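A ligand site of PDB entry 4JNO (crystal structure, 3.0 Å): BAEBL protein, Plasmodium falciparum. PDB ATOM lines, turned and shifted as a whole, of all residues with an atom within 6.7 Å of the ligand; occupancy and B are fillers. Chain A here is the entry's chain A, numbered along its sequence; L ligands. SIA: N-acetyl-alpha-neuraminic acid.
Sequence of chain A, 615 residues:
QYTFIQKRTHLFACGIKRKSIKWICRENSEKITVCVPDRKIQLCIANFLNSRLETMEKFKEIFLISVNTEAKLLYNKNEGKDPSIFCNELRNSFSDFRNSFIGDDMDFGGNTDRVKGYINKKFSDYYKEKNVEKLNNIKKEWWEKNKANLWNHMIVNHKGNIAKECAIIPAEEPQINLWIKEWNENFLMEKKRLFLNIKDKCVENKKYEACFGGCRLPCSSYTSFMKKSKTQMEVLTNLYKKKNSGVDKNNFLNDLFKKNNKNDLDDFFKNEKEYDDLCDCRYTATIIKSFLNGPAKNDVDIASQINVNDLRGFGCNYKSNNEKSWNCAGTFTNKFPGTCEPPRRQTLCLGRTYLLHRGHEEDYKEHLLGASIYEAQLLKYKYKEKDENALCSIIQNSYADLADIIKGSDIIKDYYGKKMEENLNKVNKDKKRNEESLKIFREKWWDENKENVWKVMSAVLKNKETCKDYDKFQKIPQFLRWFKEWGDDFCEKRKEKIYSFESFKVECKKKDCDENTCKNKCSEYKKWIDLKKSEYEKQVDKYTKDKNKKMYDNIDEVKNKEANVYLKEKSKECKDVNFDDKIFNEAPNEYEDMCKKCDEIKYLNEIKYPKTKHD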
ATOM      1  N   LEU A 311       4.503  -3.536   9.955  1.00  0.00           N
ATOM      2  CA  LEU A 311       5.589  -4.189  10.682  1.00  0.00           C
ATOM      3  C   LEU A 311       6.881  -3.391  10.568  1.00  0.00           C
ATOM      4  O   LEU A 311       7.442  -2.951  11.564  1.00  0.00           O
ATOM      5  CB  LEU A 311       5.799  -5.604  10.145  1.00  0.00           C
ATOM      6  CG  LEU A 311       7.031  -6.336  10.685  1.00  0.00           C
ATOM      7  CD1 LEU A 311       6.938  -6.500  12.200  1.00  0.00           C
ATOM      8  CD2 LEU A 311       7.194  -7.688  10.011  1.00  0.00           C
ATOM      9  N   GLY A 315       9.288  -0.828  12.942  1.00  0.00           N
ATOM     10  CA  GLY A 315      10.721  -1.011  13.125  1.00  0.00           C
ATOM     11  C   GLY A 315      11.094  -2.435  13.480  1.00  0.00           C
ATOM     12  O   GLY A 315      11.877  -2.678  14.394  1.00  0.00           O
ATOM     13  N   CYS A 316      10.520  -3.387  12.750  1.00  0.00           N
ATOM     14  CA  CYS A 316      10.822  -4.797  12.969  1.00  0.00           C
ATOM     15  C   CYS A 316      10.791  -5.575  11.659  1.00  0.00           C
ATOM     16  O   CYS A 316      10.360  -5.058  10.622  1.00  0.00           O
ATOM     17  CB  CYS A 316       9.821  -5.408  13.957  1.00  0.00           C
ATOM     18  SG  CYS A 316       9.935  -4.737  15.634  1.00  0.00           S
ATOM     19  N   ASN A 317      11.249  -6.820  11.704  1.00  0.00           N
ATOM     20  CA  ASN A 317      11.325  -7.646  10.506  1.00  0.00           C
ATOM     21  C   ASN A 317      11.182  -9.127  10.845  1.00  0.00           C
ATOM     22  O   ASN A 317      11.456  -9.550  11.970  1.00  0.00           O
ATOM     23  CB  ASN A 317      12.654  -7.413   9.782  1.00  0.00           C
ATOM     24  CG  ASN A 317      12.767  -8.200   8.488  1.00  0.00           C
ATOM     25  OD1 ASN A 317      11.753  -8.522   7.857  1.00  0.00           O
ATOM     26  ND2 ASN A 317      13.987  -8.518   8.090  1.00  0.00           N
ATOM     27  N   TYR A 318      10.751  -9.922   9.865  1.00  0.00           N
ATOM     28  CA  TYR A 318      10.592 -11.361  10.048  1.00  0.00           C
ATOM     29  C   TYR A 318      11.836 -11.975  10.673  1.00  0.00           C
ATOM     30  O   TYR A 318      12.953 -11.530  10.410  1.00  0.00           O
ATOM     31  CB  TYR A 318      10.289 -12.039   8.712  1.00  0.00           C
ATOM     32  CG  TYR A 318       8.931 -11.707   8.141  1.00  0.00           C
ATOM     33  CD1 TYR A 318       7.807 -12.424   8.516  1.00  0.00           C
ATOM     34  CD2 TYR A 318       8.772 -10.685   7.216  1.00  0.00           C
ATOM     35  CE1 TYR A 318       6.560 -12.130   7.987  1.00  0.00           C
ATOM     36  CE2 TYR A 318       7.541 -10.384   6.683  1.00  0.00           C
ATOM     37  CZ  TYR A 318       6.431 -11.110   7.073  1.00  0.00           C
ATOM     38  OH  TYR A 318       5.192 -10.815   6.551  1.00  0.00           O
ATOM     39  N   LYS A 319      11.634 -13.002  11.485  1.00  0.00           N
ATOM     40  CA  LYS A 319      12.743 -13.724  12.095  1.00  0.00           C
ATOM     41  C   LYS A 319      13.528 -14.453  11.019  1.00  0.00           C
ATOM     42  O   LYS A 319      13.039 -15.422  10.424  1.00  0.00           O
ATOM     43  CB  LYS A 319      12.230 -14.716  13.140  1.00  0.00           C
ATOM     44  CG  LYS A 319      11.375 -14.097  14.233  1.00  0.00           C
ATOM     45  CD  LYS A 319      12.133 -13.019  14.995  1.00  0.00           C
ATOM     46  CE  LYS A 319      11.272 -12.397  16.095  1.00  0.00           C
ATOM     47  NZ  LYS A 319      11.983 -11.328  16.835  1.00  0.00           N
ATOM     48  N   LYS A 324      20.968 -17.615  14.735  1.00  0.00           N
ATOM     49  CA  LYS A 324      22.082 -16.950  15.400  1.00  0.00           C
ATOM     50  C   LYS A 324      22.542 -17.762  16.603  1.00  0.00           C
ATOM     51  O   LYS A 324      21.724 -18.375  17.291  1.00  0.00           O
ATOM     52  CB  LYS A 324      21.678 -15.541  15.843  1.00  0.00           C
ATOM     53  CG  LYS A 324      21.315 -14.613  14.701  1.00  0.00           C
ATOM     54  CD  LYS A 324      20.832 -13.265  15.213  1.00  0.00           C
ATOM     55  CE  LYS A 324      21.908 -12.544  16.015  1.00  0.00           C
ATOM     56  NZ  LYS A 324      21.426 -11.228  16.528  1.00  0.00           N
ATOM     57  N   GLU A 341      22.750 -15.006  26.046  1.00  0.00           N
ATOM     58  CA  GLU A 341      21.560 -14.364  25.511  1.00  0.00           C
ATOM     59  C   GLU A 341      20.908 -15.232  24.444  1.00  0.00           C
ATOM     60  O   GLU A 341      21.535 -15.549  23.427  1.00  0.00           O
ATOM     61  CB  GLU A 341      21.917 -13.002  24.922  1.00  0.00           C
ATOM     62  CG  GLU A 341      20.718 -12.190  24.459  1.00  0.00           C
ATOM     63  CD  GLU A 341      21.117 -10.842  23.883  1.00  0.00           C
ATOM     64  OE1 GLU A 341      22.335 -10.573  23.797  1.00  0.00           O
ATOM     65  OE2 GLU A 341      20.214 -10.064  23.507  1.00  0.00           O
ATOM     66  N   PRO A 343      19.039 -16.375  21.207  1.00  0.00           N
ATOM     67  CA  PRO A 343      18.889 -15.757  19.882  1.00  0.00           C
ATOM     68  C   PRO A 343      17.557 -15.038  19.748  1.00  0.00           C
ATOM     69  O   PRO A 343      17.477 -13.994  19.088  1.00  0.00           O
ATOM     70  CB  PRO A 343      18.947 -16.953  18.927  1.00  0.00           C
ATOM     71  CG  PRO A 343      19.775 -17.953  19.653  1.00  0.00           C
ATOM     72  CD  PRO A 343      19.466 -17.781  21.115  1.00  0.00           C
ATOM     73  N   ARG A 344      16.514 -15.594  20.358  1.00  0.00           N
ATOM     74  CA  ARG A 344      15.202 -14.974  20.366  1.00  0.00           C
ATOM     75  C   ARG A 344      15.258 -13.599  21.024  1.00  0.00           C
ATOM     76  O   ARG A 344      14.684 -12.630  20.514  1.00  0.00           O
ATOM     77  CB  ARG A 344      14.207 -15.865  21.121  1.00  0.00           C
ATOM     78  CG  ARG A 344      12.824 -15.259  21.296  1.00  0.00           C
ATOM     79  CD  ARG A 344      12.014 -16.053  22.305  1.00  0.00           C
ATOM     80  NE  ARG A 344      12.745 -16.229  23.561  1.00  0.00           N
ATOM     81  CZ  ARG A 344      12.921 -15.274  24.475  1.00  0.00           C
ATOM     82  NH1 ARG A 344      12.425 -14.065  24.289  1.00  0.00           N
ATOM     83  NH2 ARG A 344      13.604 -15.540  25.576  1.00  0.00           N
ATOM     84  N   ARG A 345      15.949 -13.522  22.148  1.00  0.00           N
ATOM     85  CA  ARG A 345      16.096 -12.267  22.880  1.00  0.00           C
ATOM     86  C   ARG A 345      16.886 -11.254  22.064  1.00  0.00           C
ATOM     87  O   ARG A 345      16.589 -10.051  22.078  1.00  0.00           O
ATOM     88  CB  ARG A 345      16.785 -12.505  24.224  1.00  0.00           C
ATOM     89  CG  ARG A 345      17.166 -11.233  24.968  1.00  0.00           C
ATOM     90  CD  ARG A 345      15.946 -10.368  25.253  1.00  0.00           C
ATOM     91  NE  ARG A 345      16.303  -9.130  25.937  1.00  0.00           N
ATOM     92  CZ  ARG A 345      16.706  -8.018  25.314  1.00  0.00           C
ATOM     93  NH1 ARG A 345      16.811  -7.976  24.000  1.00  0.00           N
ATOM     94  NH2 ARG A 345      17.007  -6.940  26.032  1.00  0.00           N
ATOM     95  N   GLN A 346      17.898 -11.735  21.351  1.00  0.00           N
ATOM     96  CA  GLN A 346      18.763 -10.868  20.551  1.00  0.00           C
ATOM     97  C   GLN A 346      17.961 -10.128  19.488  1.00  0.00           C
ATOM     98  O   GLN A 346      18.363  -9.067  19.012  1.00  0.00           O
ATOM     99  CB  GLN A 346      19.867 -11.688  19.883  1.00  0.00           C
ATOM    100  CG  GLN A 346      20.761 -12.449  20.853  1.00  0.00           C
ATOM    101  CD  GLN A 346      21.827 -13.263  20.151  1.00  0.00           C
ATOM    102  OE1 GLN A 346      22.445 -12.789  19.199  1.00  0.00           O
ATOM    103  NE2 GLN A 346      22.043 -14.482  20.615  1.00  0.00           N
ATOM    104  N   THR A 347      16.816 -10.701  19.118  1.00  0.00           N
ATOM    105  CA  THR A 347      15.984 -10.123  18.059  1.00  0.00           C
ATOM    106  C   THR A 347      14.582  -9.775  18.565  1.00  0.00           C
ATOM    107  O   THR A 347      13.640  -9.691  17.778  1.00  0.00           O
ATOM    108  CB  THR A 347      15.844 -11.108  16.884  1.00  0.00           C
ATOM    109  OG1 THR A 347      14.957 -12.182  17.256  1.00  0.00           O
ATOM    110  CG2 THR A 347      17.198 -11.685  16.505  1.00  0.00           C
ATOM    111  N   LEU A 348      14.448  -9.581  19.877  1.00  0.00           N
ATOM    112  CA  LEU A 348      13.166  -9.237  20.473  1.00  0.00           C
ATOM    113  C   LEU A 348      12.672  -7.891  19.925  1.00  0.00           C
ATOM    114  O   LEU A 348      13.343  -6.877  20.059  1.00  0.00           O
ATOM    115  CB  LEU A 348      13.288  -9.172  21.990  1.00  0.00           C
ATOM    116  CG  LEU A 348      11.980  -8.985  22.758  1.00  0.00           C
ATOM    117  CD1 LEU A 348      11.130 -10.250  22.677  1.00  0.00           C
ATOM    118  CD2 LEU A 348      12.242  -8.606  24.203  1.00  0.00           C
ATOM    119  N   CYS A 349      11.482  -7.897  19.339  1.00  0.00           N
ATOM    120  CA  CYS A 349      10.922  -6.697  18.728  1.00  0.00           C
ATOM    121  C   CYS A 349      10.607  -5.633  19.770  1.00  0.00           C
ATOM    122  O   CYS A 349       9.781  -5.841  20.651  1.00  0.00           O
ATOM    123  CB  CYS A 349       9.655  -7.046  17.934  1.00  0.00           C
ATOM    124  SG  CYS A 349       8.876  -5.638  17.114  1.00  0.00           S
ATOM    125  N   LEU A 350      11.285  -4.490  19.661  1.00  0.00           N
ATOM    126  CA  LEU A 350      11.031  -3.357  20.545  1.00  0.00           C
ATOM    127  C   LEU A 350      10.565  -2.129  19.753  1.00  0.00           C
ATOM    128  O   LEU A 350       9.815  -1.294  20.274  1.00  0.00           O
ATOM    129  CB  LEU A 350      12.287  -3.027  21.338  1.00  0.00           C
ATOM    130  CG  LEU A 350      12.823  -4.169  22.209  1.00  0.00           C
ATOM    131  CD1 LEU A 350      14.136  -3.758  22.877  1.00  0.00           C
ATOM    132  CD2 LEU A 350      11.803  -4.592  23.251  1.00  0.00           C
ATOM    133  N   GLY A 351      11.005  -2.009  18.498  1.00  0.00           N
ATOM    134  CA  GLY A 351      10.564  -0.936  17.628  1.00  0.00           C
ATOM    135  C   GLY A 351      11.382   0.336  17.748  1.00  0.00           C
ATOM    136  O   GLY A 351      12.404   0.369  18.442  1.00  0.00           O
ATOM    137  N   ARG A 352      10.939   1.378  17.056  1.00  0.00           N
ATOM    138  CA  ARG A 352      11.598   2.679  17.083  1.00  0.00           C
ATOM    139  C   ARG A 352      10.598   3.771  17.473  1.00  0.00           C
ATOM    140  O   ARG A 352      10.417   4.063  18.660  1.00  0.00           O
ATOM    141  CB  ARG A 352      12.234   3.001  15.728  1.00  0.00           C
ATOM    142  CG  ARG A 352      11.467   2.458  14.518  1.00  0.00           C
ATOM    143  CD  ARG A 352      11.866   3.180  13.243  1.00  0.00           C
ATOM    144  NE  ARG A 352      11.427   2.459  12.045  1.00  0.00           N
ATOM    145  CZ  ARG A 352      11.746   2.815  10.805  1.00  0.00           C
ATOM    146  NH1 ARG A 352      12.506   3.891  10.587  1.00  0.00           N
ATOM    147  NH2 ARG A 352      11.307   2.113   9.779  1.00  0.00           N
ATOM    148  N   LEU A 378       5.404 -12.444  14.671  1.00  0.00           N
ATOM    149  CA  LEU A 378       6.639 -12.915  14.047  1.00  0.00           C
ATOM    150  C   LEU A 378       7.006 -14.312  14.565  1.00  0.00           C
ATOM    151  O   LEU A 378       7.428 -15.164  13.799  1.00  0.00           O
ATOM    152  CB  LEU A 378       7.780 -11.937  14.322  1.00  0.00           C
ATOM    153  CG  LEU A 378       7.602 -10.520  13.763  1.00  0.00           C
ATOM    154  CD1 LEU A 378       8.821  -9.668  14.048  1.00  0.00           C
ATOM    155  CD2 LEU A 378       7.299 -10.557  12.273  1.00  0.00           C
ATOM    156  N   ASP A 414      20.815  -4.052  26.264  1.00  0.00           N
ATOM    157  CA  ASP A 414      21.214  -3.656  24.923  1.00  0.00           C
ATOM    158  C   ASP A 414      20.702  -2.253  24.598  1.00  0.00           C
ATOM    159  O   ASP A 414      19.951  -1.668  25.378  1.00  0.00           O
ATOM    160  CB  ASP A 414      20.705  -4.656  23.883  1.00  0.00           C
ATOM    161  CG  ASP A 414      19.203  -4.795  23.892  1.00  0.00           C
ATOM    162  OD1 ASP A 414      18.516  -3.963  23.248  1.00  0.00           O
ATOM    163  OD2 ASP A 414      18.690  -5.735  24.539  1.00  0.00           O
ATOM    164  N   TYR A 415      21.123  -1.728  23.455  1.00  0.00           N
ATOM    165  CA  TYR A 415      20.756  -0.371  23.052  1.00  0.00           C
ATOM    166  C   TYR A 415      19.258  -0.133  23.164  1.00  0.00           C
ATOM    167  O   TYR A 415      18.804   0.690  23.956  1.00  0.00           O
ATOM    168  CB  TYR A 415      21.221  -0.095  21.626  1.00  0.00           C
ATOM    169  CG  TYR A 415      20.913   1.299  21.132  1.00  0.00           C
ATOM    170  CD1 TYR A 415      19.697   1.589  20.534  1.00  0.00           C
ATOM    171  CD2 TYR A 415      21.838   2.326  21.270  1.00  0.00           C
ATOM    172  CE1 TYR A 415      19.407   2.869  20.092  1.00  0.00           C
ATOM    173  CE2 TYR A 415      21.562   3.603  20.827  1.00  0.00           C
ATOM    174  CZ  TYR A 415      20.341   3.864  20.238  1.00  0.00           C
ATOM    175  OH  TYR A 415      20.065   5.141  19.794  1.00  0.00           O
ATOM    176  N   TYR A 416      18.484  -0.853  22.357  1.00  0.00           N
ATOM    177  CA  TYR A 416      17.034  -0.702  22.340  1.00  0.00           C
ATOM    178  C   TYR A 416      16.406  -1.191  23.636  1.00  0.00           C
ATOM    179  O   TYR A 416      15.285  -0.823  23.972  1.00  0.00           O
ATOM    180  CB  TYR A 416      16.434  -1.440  21.135  1.00  0.00           C
ATOM    181  CG  TYR A 416      16.861  -0.855  19.806  1.00  0.00           C
ATOM    182  CD1 TYR A 416      16.140   0.168  19.217  1.00  0.00           C
ATOM    183  CD2 TYR A 416      17.984  -1.339  19.147  1.00  0.00           C
ATOM    184  CE1 TYR A 416      16.521   0.698  17.996  1.00  0.00           C
ATOM    185  CE2 TYR A 416      18.372  -0.808  17.933  1.00  0.00           C
ATOM    186  CZ  TYR A 416      17.637   0.212  17.361  1.00  0.00           C
ATOM    187  OH  TYR A 416      18.026   0.742  16.147  1.00  0.00           O
ATOM    188  N   GLY A 417      17.141  -2.028  24.364  1.00  0.00           N
ATOM    189  CA  GLY A 417      16.690  -2.501  25.666  1.00  0.00           C
ATOM    190  C   GLY A 417      16.609  -1.356  26.652  1.00  0.00           C
ATOM    191  O   GLY A 417      15.575  -1.114  27.256  1.00  0.00           O
HETATM  192  C1  SIA L   1      14.194  -6.812  13.831  1.00  0.00           C
HETATM  193  C2  SIA L   1      15.023  -5.615  14.243  1.00  0.00           C
HETATM  194  C3  SIA L   1      14.260  -4.794  15.285  1.00  0.00           C
HETATM  195  C4  SIA L   1      14.341  -5.418  16.663  1.00  0.00           C
HETATM  196  C5  SIA L   1      15.801  -5.599  17.049  1.00  0.00           C
HETATM  197  C6  SIA L   1      16.476  -6.521  16.045  1.00  0.00           C
HETATM  198  C7  SIA L   1      17.974  -6.646  16.285  1.00  0.00           C
HETATM  199  C8  SIA L   1      18.564  -7.638  15.281  1.00  0.00           C
HETATM  200  C9  SIA L   1      19.996  -8.002  15.638  1.00  0.00           C
HETATM  201  C10 SIA L   1      16.768  -5.856  19.318  1.00  0.00           C
HETATM  202  C11 SIA L   1      17.800  -4.804  19.024  1.00  0.00           C
HETATM  203  N5  SIA L   1      15.866  -6.171  18.378  1.00  0.00           N
HETATM  204  O1A SIA L   1      14.551  -7.941  14.210  1.00  0.00           O
HETATM  205  O1B SIA L   1      13.177  -6.617  13.126  1.00  0.00           O
HETATM  206  O2  SIA L   1      15.238  -4.796  13.088  1.00  0.00           O
HETATM  207  O4  SIA L   1      13.678  -4.561  17.596  1.00  0.00           O
HETATM  208  O6  SIA L   1      16.293  -6.108  14.684  1.00  0.00           O
HETATM  209  O7  SIA L   1      18.600  -5.374  16.118  1.00  0.00           O
HETATM  210  O8  SIA L   1      17.768  -8.823  15.252  1.00  0.00           O
HETATM  211  O9  SIA L   1      20.060  -8.507  16.979  1.00  0.00           O
HETATM  212  O10 SIA L   1      16.744  -6.399  20.406  1.00  0.00           O
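Residues that only touch the ligand: Gly 315 (3.3 Å), Cys 316 (3.0 Å), Arg 345 (3.9 Å), Thr 347 (3.2 Å), Cys 349 (3.7 Å), Gly 351 (3.8 Å) and Tyr 416 (3.5 Å).
Hydrophobic or aromatic side chains within 4 Å of the ligand: Tyr 416.
An oxygen (O4) of the ligand sits at hydrogen-bond distance from the backbone NH (N) of Leu 350, 3.2 Å away.
An oxygen (O1B) of the ligand lies within hydrogen-bond range of the backbone NH of Asn 317 (2.4 Å).
The backbone carbonyl oxygen (O) of Gln 346 lies within hydrogen-bond range of an oxygen (O9) of the ligand (2.7 Å).
The side-chain amino group (NZ) of Lys 324 is in hydrogen-bond range of an oxygen (O9) of the ligand.
O of Leu 348 is in hydrogen-bond range of N5 of the ligand (3.1 Å).
The backbone NH of Cys 316 lies within hydrogen-bond range of the backbone carbonyl oxygen of Leu 311, at 3.3 Å.
The side-chain amide nitrogen (NE2) of Gln 346 is in hydrogen-bond range of the backbone carbonyl oxygen (O) of Glu 341, at 3.1 Å.
The side-chain amino group (NZ) of Lys 324 lies close to the side-chain amide oxygen (OE1) of Gln 346, at 3.3 Å.
The backbone carbonyl oxygen (O) of Thr 347 sits at hydrogen-bond distance from the side-chain amino group (NZ) of Lys 319, 2.5 Å away.
The backbone carbonyl oxygen (O) of Arg 344 lies within hydrogen-bond range of the side-chain hydroxyl (OG1) of Thr 347 (3.3 Å).
The side-chain carboxylate (OD2) of Asp 414 lies within salt-bridge range of the guanidinium group (NH2) of Arg 345 (2.6 Å).
SG of Cys 316 is disulfide-bonded to SG of Cys 349 (2.0 Å).
The backbone NH (N) of Tyr 416 is in hydrogen-bond range of the side-chain carboxylate (OD1) of Asp 414.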
